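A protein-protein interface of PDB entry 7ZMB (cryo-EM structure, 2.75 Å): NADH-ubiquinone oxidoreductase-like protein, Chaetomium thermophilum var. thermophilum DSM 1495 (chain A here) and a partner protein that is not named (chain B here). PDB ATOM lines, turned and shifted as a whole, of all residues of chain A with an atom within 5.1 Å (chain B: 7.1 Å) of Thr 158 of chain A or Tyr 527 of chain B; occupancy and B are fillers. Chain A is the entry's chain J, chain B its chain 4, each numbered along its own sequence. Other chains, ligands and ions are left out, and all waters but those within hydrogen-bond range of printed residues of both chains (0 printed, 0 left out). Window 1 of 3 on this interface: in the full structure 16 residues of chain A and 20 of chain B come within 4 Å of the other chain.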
ATOM      1  N   PRO A 154      -5.604  37.238  18.623  1.00  0.00           N
ATOM      2  CA  PRO A 154      -4.782  37.986  17.668  1.00  0.00           C
ATOM      3  C   PRO A 154      -4.120  37.056  16.667  1.00  0.00           C
ATOM      4  O   PRO A 154      -3.742  35.930  16.989  1.00  0.00           O
ATOM      5  CB  PRO A 154      -3.755  38.689  18.560  1.00  0.00           C
ATOM      6  CG  PRO A 154      -3.720  37.884  19.799  1.00  0.00           C
ATOM      7  CD  PRO A 154      -5.111  37.387  20.001  1.00  0.00           C
ATOM      8  N   ILE A 155      -3.978  37.550  15.436  1.00  0.00           N
ATOM      9  CA  ILE A 155      -3.463  36.721  14.355  1.00  0.00           C
ATOM     10  C   ILE A 155      -2.058  36.231  14.666  1.00  0.00           C
ATOM     11  O   ILE A 155      -1.654  35.156  14.213  1.00  0.00           O
ATOM     12  CB  ILE A 155      -3.522  37.498  13.027  1.00  0.00           C
ATOM     13  CG1 ILE A 155      -3.081  36.614  11.864  1.00  0.00           C
ATOM     14  CG2 ILE A 155      -2.673  38.759  13.102  1.00  0.00           C
ATOM     15  CD1 ILE A 155      -4.039  35.518  11.549  1.00  0.00           C
ATOM     16  N   GLU A 156      -1.298  36.990  15.456  1.00  0.00           N
ATOM     17  CA  GLU A 156       0.051  36.560  15.802  1.00  0.00           C
ATOM     18  C   GLU A 156       0.030  35.247  16.570  1.00  0.00           C
ATOM     19  O   GLU A 156       0.884  34.380  16.358  1.00  0.00           O
ATOM     20  CB  GLU A 156       0.751  37.648  16.616  1.00  0.00           C
ATOM     21  N   GLU A 157      -0.945  35.082  17.464  1.00  0.00           N
ATOM     22  CA  GLU A 157      -0.973  33.908  18.326  1.00  0.00           C
ATOM     23  C   GLU A 157      -1.148  32.627  17.522  1.00  0.00           C
ATOM     24  O   GLU A 157      -0.475  31.625  17.789  1.00  0.00           O
ATOM     25  CB  GLU A 157      -2.081  34.054  19.367  1.00  0.00           C
ATOM     26  CG  GLU A 157      -2.143  32.918  20.369  1.00  0.00           C
ATOM     27  CD  GLU A 157      -3.219  33.130  21.414  1.00  0.00           C
ATOM     28  OE1 GLU A 157      -3.927  34.155  21.336  1.00  0.00           O
ATOM     29  OE2 GLU A 157      -3.358  32.272  22.310  1.00  0.00           O
ATOM     30  N   THR A 158      -2.048  32.631  16.536  1.00  0.00           N
ATOM     31  CA  THR A 158      -2.197  31.444  15.701  1.00  0.00           C
ATOM     32  C   THR A 158      -0.974  31.230  14.821  1.00  0.00           C
ATOM     33  O   THR A 158      -0.529  30.092  14.640  1.00  0.00           O
ATOM     34  CB  THR A 158      -3.471  31.525  14.853  1.00  0.00           C
ATOM     35  OG1 THR A 158      -3.613  30.322  14.085  1.00  0.00           O
ATOM     36  CG2 THR A 158      -3.447  32.708  13.912  1.00  0.00           C
ATOM     37  N   LEU A 159      -0.402  32.305  14.280  1.00  0.00           N
ATOM     38  CA  LEU A 159       0.749  32.145  13.402  1.00  0.00           C
ATOM     39  C   LEU A 159       1.927  31.544  14.151  1.00  0.00           C
ATOM     40  O   LEU A 159       2.653  30.708  13.605  1.00  0.00           O
ATOM     41  CB  LEU A 159       1.130  33.481  12.768  1.00  0.00           C
ATOM     42  CG  LEU A 159       0.099  34.142  11.854  1.00  0.00           C
ATOM     43  CD1 LEU A 159       0.779  35.117  10.907  1.00  0.00           C
ATOM     44  CD2 LEU A 159      -0.691  33.110  11.076  1.00  0.00           C
ATOM     45  N   ALA A 160       2.130  31.952  15.402  1.00  0.00           N
ATOM     46  CA  ALA A 160       3.161  31.325  16.212  1.00  0.00           C
ATOM     47  C   ALA A 160       2.876  29.853  16.436  1.00  0.00           C
ATOM     48  O   ALA A 160       3.809  29.071  16.635  1.00  0.00           O
ATOM     49  CB  ALA A 160       3.288  32.045  17.552  1.00  0.00           C
ATOM     50  N   GLU A 161       1.609  29.462  16.398  1.00  0.00           N
ATOM     51  CA  GLU A 161       1.203  28.095  16.691  1.00  0.00           C
ATOM     52  C   GLU A 161       1.303  27.214  15.448  1.00  0.00           C
ATOM     53  O   GLU A 161       2.075  26.254  15.419  1.00  0.00           O
ATOM     54  CB  GLU A 161      -0.220  28.116  17.249  1.00  0.00           C
ATOM     55  CG  GLU A 161      -0.276  28.102  18.759  1.00  0.00           C
ATOM     56  CD  GLU A 161      -1.567  28.698  19.290  1.00  0.00           C
ATOM     57  OE1 GLU A 161      -2.421  29.094  18.470  1.00  0.00           O
ATOM     58  OE2 GLU A 161      -1.711  28.807  20.526  1.00  0.00           O
ATOM     59  N   ILE A 162       0.545  27.545  14.403  1.00  0.00           N
ATOM     60  CA  ILE A 162       0.470  26.697  13.223  1.00  0.00           C
ATOM     61  C   ILE A 162       1.429  27.125  12.134  1.00  0.00           C
ATOM     62  O   ILE A 162       1.573  26.413  11.133  1.00  0.00           O
ATOM     63  CB  ILE A 162      -0.964  26.635  12.669  1.00  0.00           C
ATOM     64  CG1 ILE A 162      -1.480  28.032  12.350  1.00  0.00           C
ATOM     65  CG2 ILE A 162      -1.856  25.947  13.647  1.00  0.00           C
ATOM     66  CD1 ILE A 162      -2.811  28.028  11.669  1.00  0.00           C
ATOM     67  N   GLY A 163       2.099  28.255  12.298  1.00  0.00           N
ATOM     68  CA  GLY A 163       3.038  28.703  11.302  1.00  0.00           C
ATOM     69  C   GLY A 163       2.379  29.571  10.259  1.00  0.00           C
ATOM     70  O   GLY A 163       1.583  30.453  10.583  1.00  0.00           O
ATOM     71  N   GLY A 167      -2.293  26.640   3.470  1.00  0.00           N
ATOM     72  CA  GLY A 167      -3.589  27.264   3.523  1.00  0.00           C
ATOM     73  C   GLY A 167      -3.669  28.462   4.438  1.00  0.00           C
ATOM     74  O   GLY A 167      -4.627  29.232   4.344  1.00  0.00           O
ATOM     75  N   ILE A 168      -2.698  28.631   5.328  1.00  0.00           N
ATOM     76  CA  ILE A 168      -2.631  29.828   6.178  1.00  0.00           C
ATOM     77  C   ILE A 168      -1.789  30.835   5.408  1.00  0.00           C
ATOM     78  O   ILE A 168      -0.578  30.970   5.589  1.00  0.00           O
ATOM     79  CB  ILE A 168      -2.069  29.521   7.567  1.00  0.00           C
ATOM     80  CG1 ILE A 168      -2.712  28.251   8.123  1.00  0.00           C
ATOM     81  CG2 ILE A 168      -2.297  30.688   8.498  1.00  0.00           C
ATOM     82  CD1 ILE A 168      -4.213  28.313   8.219  1.00  0.00           C
ATOM     83  N   TYR B 245      -3.900  26.087  22.228  1.00  0.00           N
ATOM     84  CA  TYR B 245      -3.211  25.163  21.341  1.00  0.00           C
ATOM     85  C   TYR B 245      -2.914  23.860  22.055  1.00  0.00           C
ATOM     86  O   TYR B 245      -3.147  22.777  21.512  1.00  0.00           O
ATOM     87  CB  TYR B 245      -1.916  25.780  20.841  1.00  0.00           C
ATOM     88  CG  TYR B 245      -1.165  24.930  19.861  1.00  0.00           C
ATOM     89  CD1 TYR B 245      -1.768  24.499  18.691  1.00  0.00           C
ATOM     90  CD2 TYR B 245       0.131  24.525  20.117  1.00  0.00           C
ATOM     91  CE1 TYR B 245      -1.086  23.717  17.781  1.00  0.00           C
ATOM     92  CE2 TYR B 245       0.822  23.735  19.220  1.00  0.00           C
ATOM     93  CZ  TYR B 245       0.206  23.332  18.054  1.00  0.00           C
ATOM     94  OH  TYR B 245       0.897  22.547  17.165  1.00  0.00           O
ATOM     95  N   GLN B 248      -6.039  21.906  22.374  1.00  0.00           N
ATOM     96  CA  GLN B 248      -6.387  21.276  21.108  1.00  0.00           C
ATOM     97  C   GLN B 248      -5.570  20.012  20.866  1.00  0.00           C
ATOM     98  O   GLN B 248      -6.113  18.997  20.420  1.00  0.00           O
ATOM     99  CB  GLN B 248      -6.208  22.273  19.970  1.00  0.00           C
ATOM    100  CG  GLN B 248      -7.405  23.179  19.799  1.00  0.00           C
ATOM    101  CD  GLN B 248      -7.212  24.205  18.724  1.00  0.00           C
ATOM    102  OE1 GLN B 248      -7.080  23.875  17.550  1.00  0.00           O
ATOM    103  NE2 GLN B 248      -7.177  25.464  19.118  1.00  0.00           N
ATOM    104  N   LEU B 304     -12.810  18.774  13.041  1.00  0.00           N
ATOM    105  CA  LEU B 304     -12.532  19.869  12.111  1.00  0.00           C
ATOM    106  C   LEU B 304     -12.929  21.233  12.659  1.00  0.00           C
ATOM    107  O   LEU B 304     -12.071  22.132  12.688  1.00  0.00           O
ATOM    108  CB  LEU B 304     -13.179  19.585  10.753  1.00  0.00           C
ATOM    109  CG  LEU B 304     -12.540  18.416  10.003  1.00  0.00           C
ATOM    110  CD1 LEU B 304     -13.106  18.286   8.590  1.00  0.00           C
ATOM    111  CD2 LEU B 304     -11.026  18.541   9.997  1.00  0.00           C
ATOM    112  N   LEU B 307     -11.119  21.866  16.565  1.00  0.00           N
ATOM    113  CA  LEU B 307      -9.678  21.676  16.754  1.00  0.00           C
ATOM    114  C   LEU B 307      -8.912  22.039  15.486  1.00  0.00           C
ATOM    115  O   LEU B 307      -8.230  21.199  14.895  1.00  0.00           O
ATOM    116  CB  LEU B 307      -9.371  20.241  17.178  1.00  0.00           C
ATOM    117  CG  LEU B 307     -10.117  19.655  18.382  1.00  0.00           C
ATOM    118  CD1 LEU B 307      -9.704  18.225  18.592  1.00  0.00           C
ATOM    119  CD2 LEU B 307      -9.843  20.466  19.627  1.00  0.00           C
ATOM    120  N   PRO B 308      -8.974  23.309  15.055  1.00  0.00           N
ATOM    121  CA  PRO B 308      -8.368  23.694  13.774  1.00  0.00           C
ATOM    122  C   PRO B 308      -6.852  23.635  13.765  1.00  0.00           C
ATOM    123  O   PRO B 308      -6.249  22.998  12.897  1.00  0.00           O
ATOM    124  CB  PRO B 308      -8.847  25.136  13.580  1.00  0.00           C
ATOM    125  CG  PRO B 308      -9.931  25.343  14.551  1.00  0.00           C
ATOM    126  CD  PRO B 308      -9.665  24.437  15.692  1.00  0.00           C
ATOM    127  N   GLN B 309      -6.233  24.314  14.732  1.00  0.00           N
ATOM    128  CA  GLN B 309      -4.782  24.284  14.864  1.00  0.00           C
ATOM    129  C   GLN B 309      -4.261  22.872  15.078  1.00  0.00           C
ATOM    130  O   GLN B 309      -3.266  22.474  14.462  1.00  0.00           O
ATOM    131  CB  GLN B 309      -4.349  25.204  16.009  1.00  0.00           C
ATOM    132  CG  GLN B 309      -4.582  26.687  15.759  1.00  0.00           C
ATOM    133  CD  GLN B 309      -5.990  27.158  16.018  1.00  0.00           C
ATOM    134  OE1 GLN B 309      -6.777  26.492  16.684  1.00  0.00           O
ATOM    135  NE2 GLN B 309      -6.321  28.320  15.474  1.00  0.00           N
ATOM    136  N   ALA B 310      -4.917  22.096  15.944  1.00  0.00           N
ATOM    137  CA  ALA B 310      -4.416  20.765  16.267  1.00  0.00           C
ATOM    138  C   ALA B 310      -4.368  19.872  15.039  1.00  0.00           C
ATOM    139  O   ALA B 310      -3.395  19.142  14.836  1.00  0.00           O
ATOM    140  CB  ALA B 310      -5.278  20.120  17.349  1.00  0.00           C
ATOM    141  N   LEU B 312      -4.175  20.815  11.841  1.00  0.00           N
ATOM    142  CA  LEU B 312      -3.238  21.304  10.838  1.00  0.00           C
ATOM    143  C   LEU B 312      -1.806  20.890  11.147  1.00  0.00           C
ATOM    144  O   LEU B 312      -0.985  20.774  10.231  1.00  0.00           O
ATOM    145  CB  LEU B 312      -3.334  22.825  10.727  1.00  0.00           C
ATOM    146  CG  LEU B 312      -2.669  23.435   9.492  1.00  0.00           C
ATOM    147  CD1 LEU B 312      -3.508  23.192   8.260  1.00  0.00           C
ATOM    148  CD2 LEU B 312      -2.416  24.910   9.688  1.00  0.00           C
ATOM    149  N   ASN B 313      -1.483  20.662  12.416  1.00  0.00           N
ATOM    150  CA  ASN B 313      -0.123  20.316  12.796  1.00  0.00           C
ATOM    151  C   ASN B 313       0.092  18.826  12.989  1.00  0.00           C
ATOM    152  O   ASN B 313       1.243  18.388  13.030  1.00  0.00           O
ATOM    153  CB  ASN B 313       0.274  21.052  14.077  1.00  0.00           C
ATOM    154  CG  ASN B 313       0.648  22.500  13.824  1.00  0.00           C
ATOM    155  OD1 ASN B 313       0.582  22.979  12.696  1.00  0.00           O
ATOM    156  ND2 ASN B 313       1.047  23.201  14.874  1.00  0.00           N
ATOM    157  N   ASN B 361      -7.943  19.423   4.582  1.00  0.00           N
ATOM    158  CA  ASN B 361      -8.275  20.848   4.642  1.00  0.00           C
ATOM    159  C   ASN B 361      -8.620  21.406   3.266  1.00  0.00           C
ATOM    160  O   ASN B 361      -8.493  22.603   3.015  1.00  0.00           O
ATOM    161  CB  ASN B 361      -7.142  21.652   5.286  1.00  0.00           C
ATOM    162  CG  ASN B 361      -7.620  22.934   5.908  1.00  0.00           C
ATOM    163  OD1 ASN B 361      -8.721  23.009   6.437  1.00  0.00           O
ATOM    164  ND2 ASN B 361      -6.790  23.961   5.843  1.00  0.00           N
ATOM    165  N   THR B 362      -9.066  20.536   2.368  1.00  0.00           N
ATOM    166  CA  THR B 362      -9.374  20.890   0.991  1.00  0.00           C
ATOM    167  C   THR B 362     -10.845  20.617   0.745  1.00  0.00           C
ATOM    168  O   THR B 362     -11.367  19.589   1.174  1.00  0.00           O
ATOM    169  CB  THR B 362      -8.514  20.085   0.004  1.00  0.00           C
ATOM    170  OG1 THR B 362      -7.134  20.419   0.180  1.00  0.00           O
ATOM    171  CG2 THR B 362      -8.912  20.374  -1.425  1.00  0.00           C
ATOM    172  N   LEU B 366     -12.547  16.822   1.337  1.00  0.00           N
ATOM    173  CA  LEU B 366     -13.630  16.595   2.287  1.00  0.00           C
ATOM    174  C   LEU B 366     -14.871  16.063   1.591  1.00  0.00           C
ATOM    175  O   LEU B 366     -15.553  15.175   2.114  1.00  0.00           O
ATOM    176  CB  LEU B 366     -13.945  17.894   3.026  1.00  0.00           C
ATOM    177  CG  LEU B 366     -12.792  18.609   3.717  1.00  0.00           C
ATOM    178  CD1 LEU B 366     -13.165  20.042   4.034  1.00  0.00           C
ATOM    179  CD2 LEU B 366     -12.398  17.881   4.963  1.00  0.00           C
ATOM    180  N   SER B 523     -18.155  23.833   3.127  1.00  0.00           N
ATOM    181  CA  SER B 523     -17.321  25.028   3.122  1.00  0.00           C
ATOM    182  C   SER B 523     -17.004  25.503   4.532  1.00  0.00           C
ATOM    183  O   SER B 523     -15.938  26.077   4.768  1.00  0.00           O
ATOM    184  CB  SER B 523     -18.032  26.131   2.345  1.00  0.00           C
ATOM    185  OG  SER B 523     -17.285  27.325   2.341  1.00  0.00           O
ATOM    186  N   SER B 524     -17.914  25.277   5.474  1.00  0.00           N
ATOM    187  CA  SER B 524     -17.739  25.732   6.846  1.00  0.00           C
ATOM    188  C   SER B 524     -16.658  24.974   7.605  1.00  0.00           C
ATOM    189  O   SER B 524     -16.243  25.435   8.671  1.00  0.00           O
ATOM    190  CB  SER B 524     -19.060  25.612   7.591  1.00  0.00           C
ATOM    191  OG  SER B 524     -19.520  24.275   7.578  1.00  0.00           O
ATOM    192  N   VAL B 525     -16.201  23.831   7.108  1.00  0.00           N
ATOM    193  CA  VAL B 525     -15.253  23.009   7.844  1.00  0.00           C
ATOM    194  C   VAL B 525     -13.843  23.120   7.265  1.00  0.00           C
ATOM    195  O   VAL B 525     -12.994  22.285   7.555  1.00  0.00           O
ATOM    196  CB  VAL B 525     -15.718  21.545   7.932  1.00  0.00           C
ATOM    197  CG1 VAL B 525     -17.126  21.473   8.487  1.00  0.00           C
ATOM    198  CG2 VAL B 525     -15.655  20.871   6.592  1.00  0.00           C
ATOM    199  N   VAL B 526     -13.577  24.152   6.470  1.00  0.00           N
ATOM    200  CA  VAL B 526     -12.230  24.429   5.995  1.00  0.00           C
ATOM    201  C   VAL B 526     -11.564  25.405   6.957  1.00  0.00           C
ATOM    202  O   VAL B 526     -12.224  26.156   7.672  1.00  0.00           O
ATOM    203  CB  VAL B 526     -12.239  24.985   4.557  1.00  0.00           C
ATOM    204  CG1 VAL B 526     -10.829  25.000   3.966  1.00  0.00           C
ATOM    205  CG2 VAL B 526     -13.191  24.197   3.677  1.00  0.00           C
ATOM    206  N   TYR B 527     -10.230  25.394   6.993  1.00  0.00           N
ATOM    207  CA  TYR B 527      -9.477  26.290   7.904  1.00  0.00           C
ATOM    208  C   TYR B 527      -8.393  27.023   7.119  1.00  0.00           C
ATOM    209  O   TYR B 527      -7.434  26.381   6.684  1.00  0.00           O
ATOM    210  CB  TYR B 527      -8.822  25.479   9.020  1.00  0.00           C
ATOM    211  CG  TYR B 527      -8.133  26.298  10.077  1.00  0.00           C
ATOM    212  CD1 TYR B 527      -8.817  27.274  10.781  1.00  0.00           C
ATOM    213  CD2 TYR B 527      -6.797  26.089  10.374  1.00  0.00           C
ATOM    214  CE1 TYR B 527      -8.188  28.026  11.757  1.00  0.00           C
ATOM    215  CE2 TYR B 527      -6.153  26.832  11.346  1.00  0.00           C
ATOM    216  CZ  TYR B 527      -6.853  27.800  12.039  1.00  0.00           C
ATOM    217  OH  TYR B 527      -6.212  28.544  12.982  1.00  0.00           O
ATOM    218  N   GLY B 528      -8.532  28.334   6.954  1.00  0.00           N
ATOM    219  CA  GLY B 528      -7.453  29.090   6.299  1.00  0.00           C
ATOM    220  C   GLY B 528      -7.959  30.316   5.582  1.00  0.00           C
ATOM    221  O   GLY B 528      -9.180  30.538   5.594  1.00  0.00           O
ATOM    222  N   ILE B 529      -7.050  31.083   4.980  1.00  0.00           N
ATOM    223  CA  ILE B 529      -7.442  32.371   4.342  1.00  0.00           C
ATOM    224  C   ILE B 529      -6.477  32.652   3.194  1.00  0.00           C
ATOM    225  O   ILE B 529      -5.369  32.105   3.215  1.00  0.00           O
ATOM    226  CB  ILE B 529      -7.406  33.521   5.368  1.00  0.00           C
ATOM    227  CG1 ILE B 529      -6.072  33.574   6.116  1.00  0.00           C
ATOM    228  CG2 ILE B 529      -8.590  33.452   6.320  1.00  0.00           C
ATOM    229  CD1 ILE B 529      -5.823  34.883   6.822  1.00  0.00           C
ATOM    230  N   TYR B 535     -10.404  39.427   5.228  1.00  0.00           N
ATOM    231  CA  TYR B 535     -10.644  40.711   5.884  1.00  0.00           C
ATOM    232  C   TYR B 535     -11.011  41.803   4.880  1.00  0.00           C
ATOM    233  O   TYR B 535     -10.452  42.902   4.890  1.00  0.00           O
ATOM    234  CB  TYR B 535      -9.433  41.127   6.718  1.00  0.00           C
ATOM    235  CG  TYR B 535      -8.906  40.034   7.604  1.00  0.00           C
ATOM    236  CD1 TYR B 535      -9.606  39.631   8.726  1.00  0.00           C
ATOM    237  CD2 TYR B 535      -7.711  39.411   7.323  1.00  0.00           C
ATOM    238  CE1 TYR B 535      -9.129  38.631   9.539  1.00  0.00           C
ATOM    239  CE2 TYR B 535      -7.228  38.412   8.130  1.00  0.00           C
ATOM    240  CZ  TYR B 535      -7.939  38.026   9.235  1.00  0.00           C
ATOM    241  OH  TYR B 535      -7.457  37.035  10.050  1.00  0.00           O
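The side-chain hydroxyl of Thr 158 of chain A is in hydrogen-bond range of the side-chain hydroxyl of Tyr 527 of chain B (3.3 Å).
O of Glu 161 of chain A lies within hydrogen-bond range of ND2 of Asn 313 of chain B, at 3.3 Å.
The backbone carbonyl oxygen (O) of Gly 167 of chain A is in hydrogen-bond range of the backbone NH (N) of Ile 529 of chain B (3.1 Å).
OE1 of Gln 309 of chain B is in hydrogen-bond range of NE2 of Gln 248 of chain B (2.7 Å).
OH of Tyr 527 of chain B is in hydrogen-bond range of NE2 of Gln 309 of chain B.
The side-chain amide nitrogen of Asn 361 of chain B lies within hydrogen-bond range of the backbone carbonyl oxygen of Tyr 527 of chain B (2.6 Å).
Among the printed residues, pairs that only touch across the chains: Glu 161 of chain A with Tyr 245 of chain B (3.1 Å), Gly 167 of chain A with Gly 528 of chain B (3.4 Å), Ile 162 of chain A with Gln 309 of chain B (3.5 Å), Ile 162 of chain A with Tyr 527 of chain B (3.6 Å), Thr 158 of chain A with Gln 309 of chain B (3.6 Å), Ile 168 of chain A with Leu 312 of chain B (3.7 Å), Ile 162 of chain A with Leu 312 of chain B (3.7 Å), Ile 162 of chain A with Asn 313 of chain B (3.8 Å), Ile 168 of chain A with Gly 528 of chain B (3.8 Å) and Ile 168 of chain A with Tyr 527 of chain B (3.97 Å).
Of chain B, only Gln 309 (3.6 Å) and Tyr 527 (3.3 Å) come within 4 Å of Thr 158 of chain A.
Of the printed residues of chain A, Tyr 527 of chain B touches Thr 158 (3.3 Å), Ile 162 (3.6 Å) and Ile 168 (3.97 Å).
Printed residues of chain A within 4 Å of Tyr 245 of chain B: Glu 161 (3.1 Å).
Printed residues of chain A within 4 Å of Gln 309 of chain B: Thr 158 and Ile 162.
Printed residues of chain B within 4 Å of Gly 167 of chain A: Gly 528 and Ile 529.
Of the printed residues of chain A, Ile 529 of chain B touches Gly 167 (3.1 Å).
Printed residues of chain A within 4 Å of Leu 312 of chain B: Ile 162 and Ile 168.
Ala 160 of chain A touches none of the printed residues of chain B.
Ala 310 of chain B touches none of the printed residues of chain A.
The nearest printed residue of chain B that does not touch Gly 167 of chain A is Tyr 527 of chain B (4.6 Å).
Of the 20 printed residues of chain B, 7 touch a printed residue of chain A.
Printed residues of chain B that touch a printed residue of chain A: Tyr 245, Gln 309, Leu 312, Asn 313, Tyr 527, Gly 528 and Ile 529.
Hydrophobic or aromatic side chains of chain B that line the printed part of chain A: Tyr 245, Leu 312 and Tyr 527.
Hydrophobic or aromatic side chains of chain A that line the printed part of chain B: Ile 162 and Ile 168.
Along chain A the printed residues that touch a printed residue of chain B span positions 158 to 168.
Among the printed residues, 13 pairs touch across the chains.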
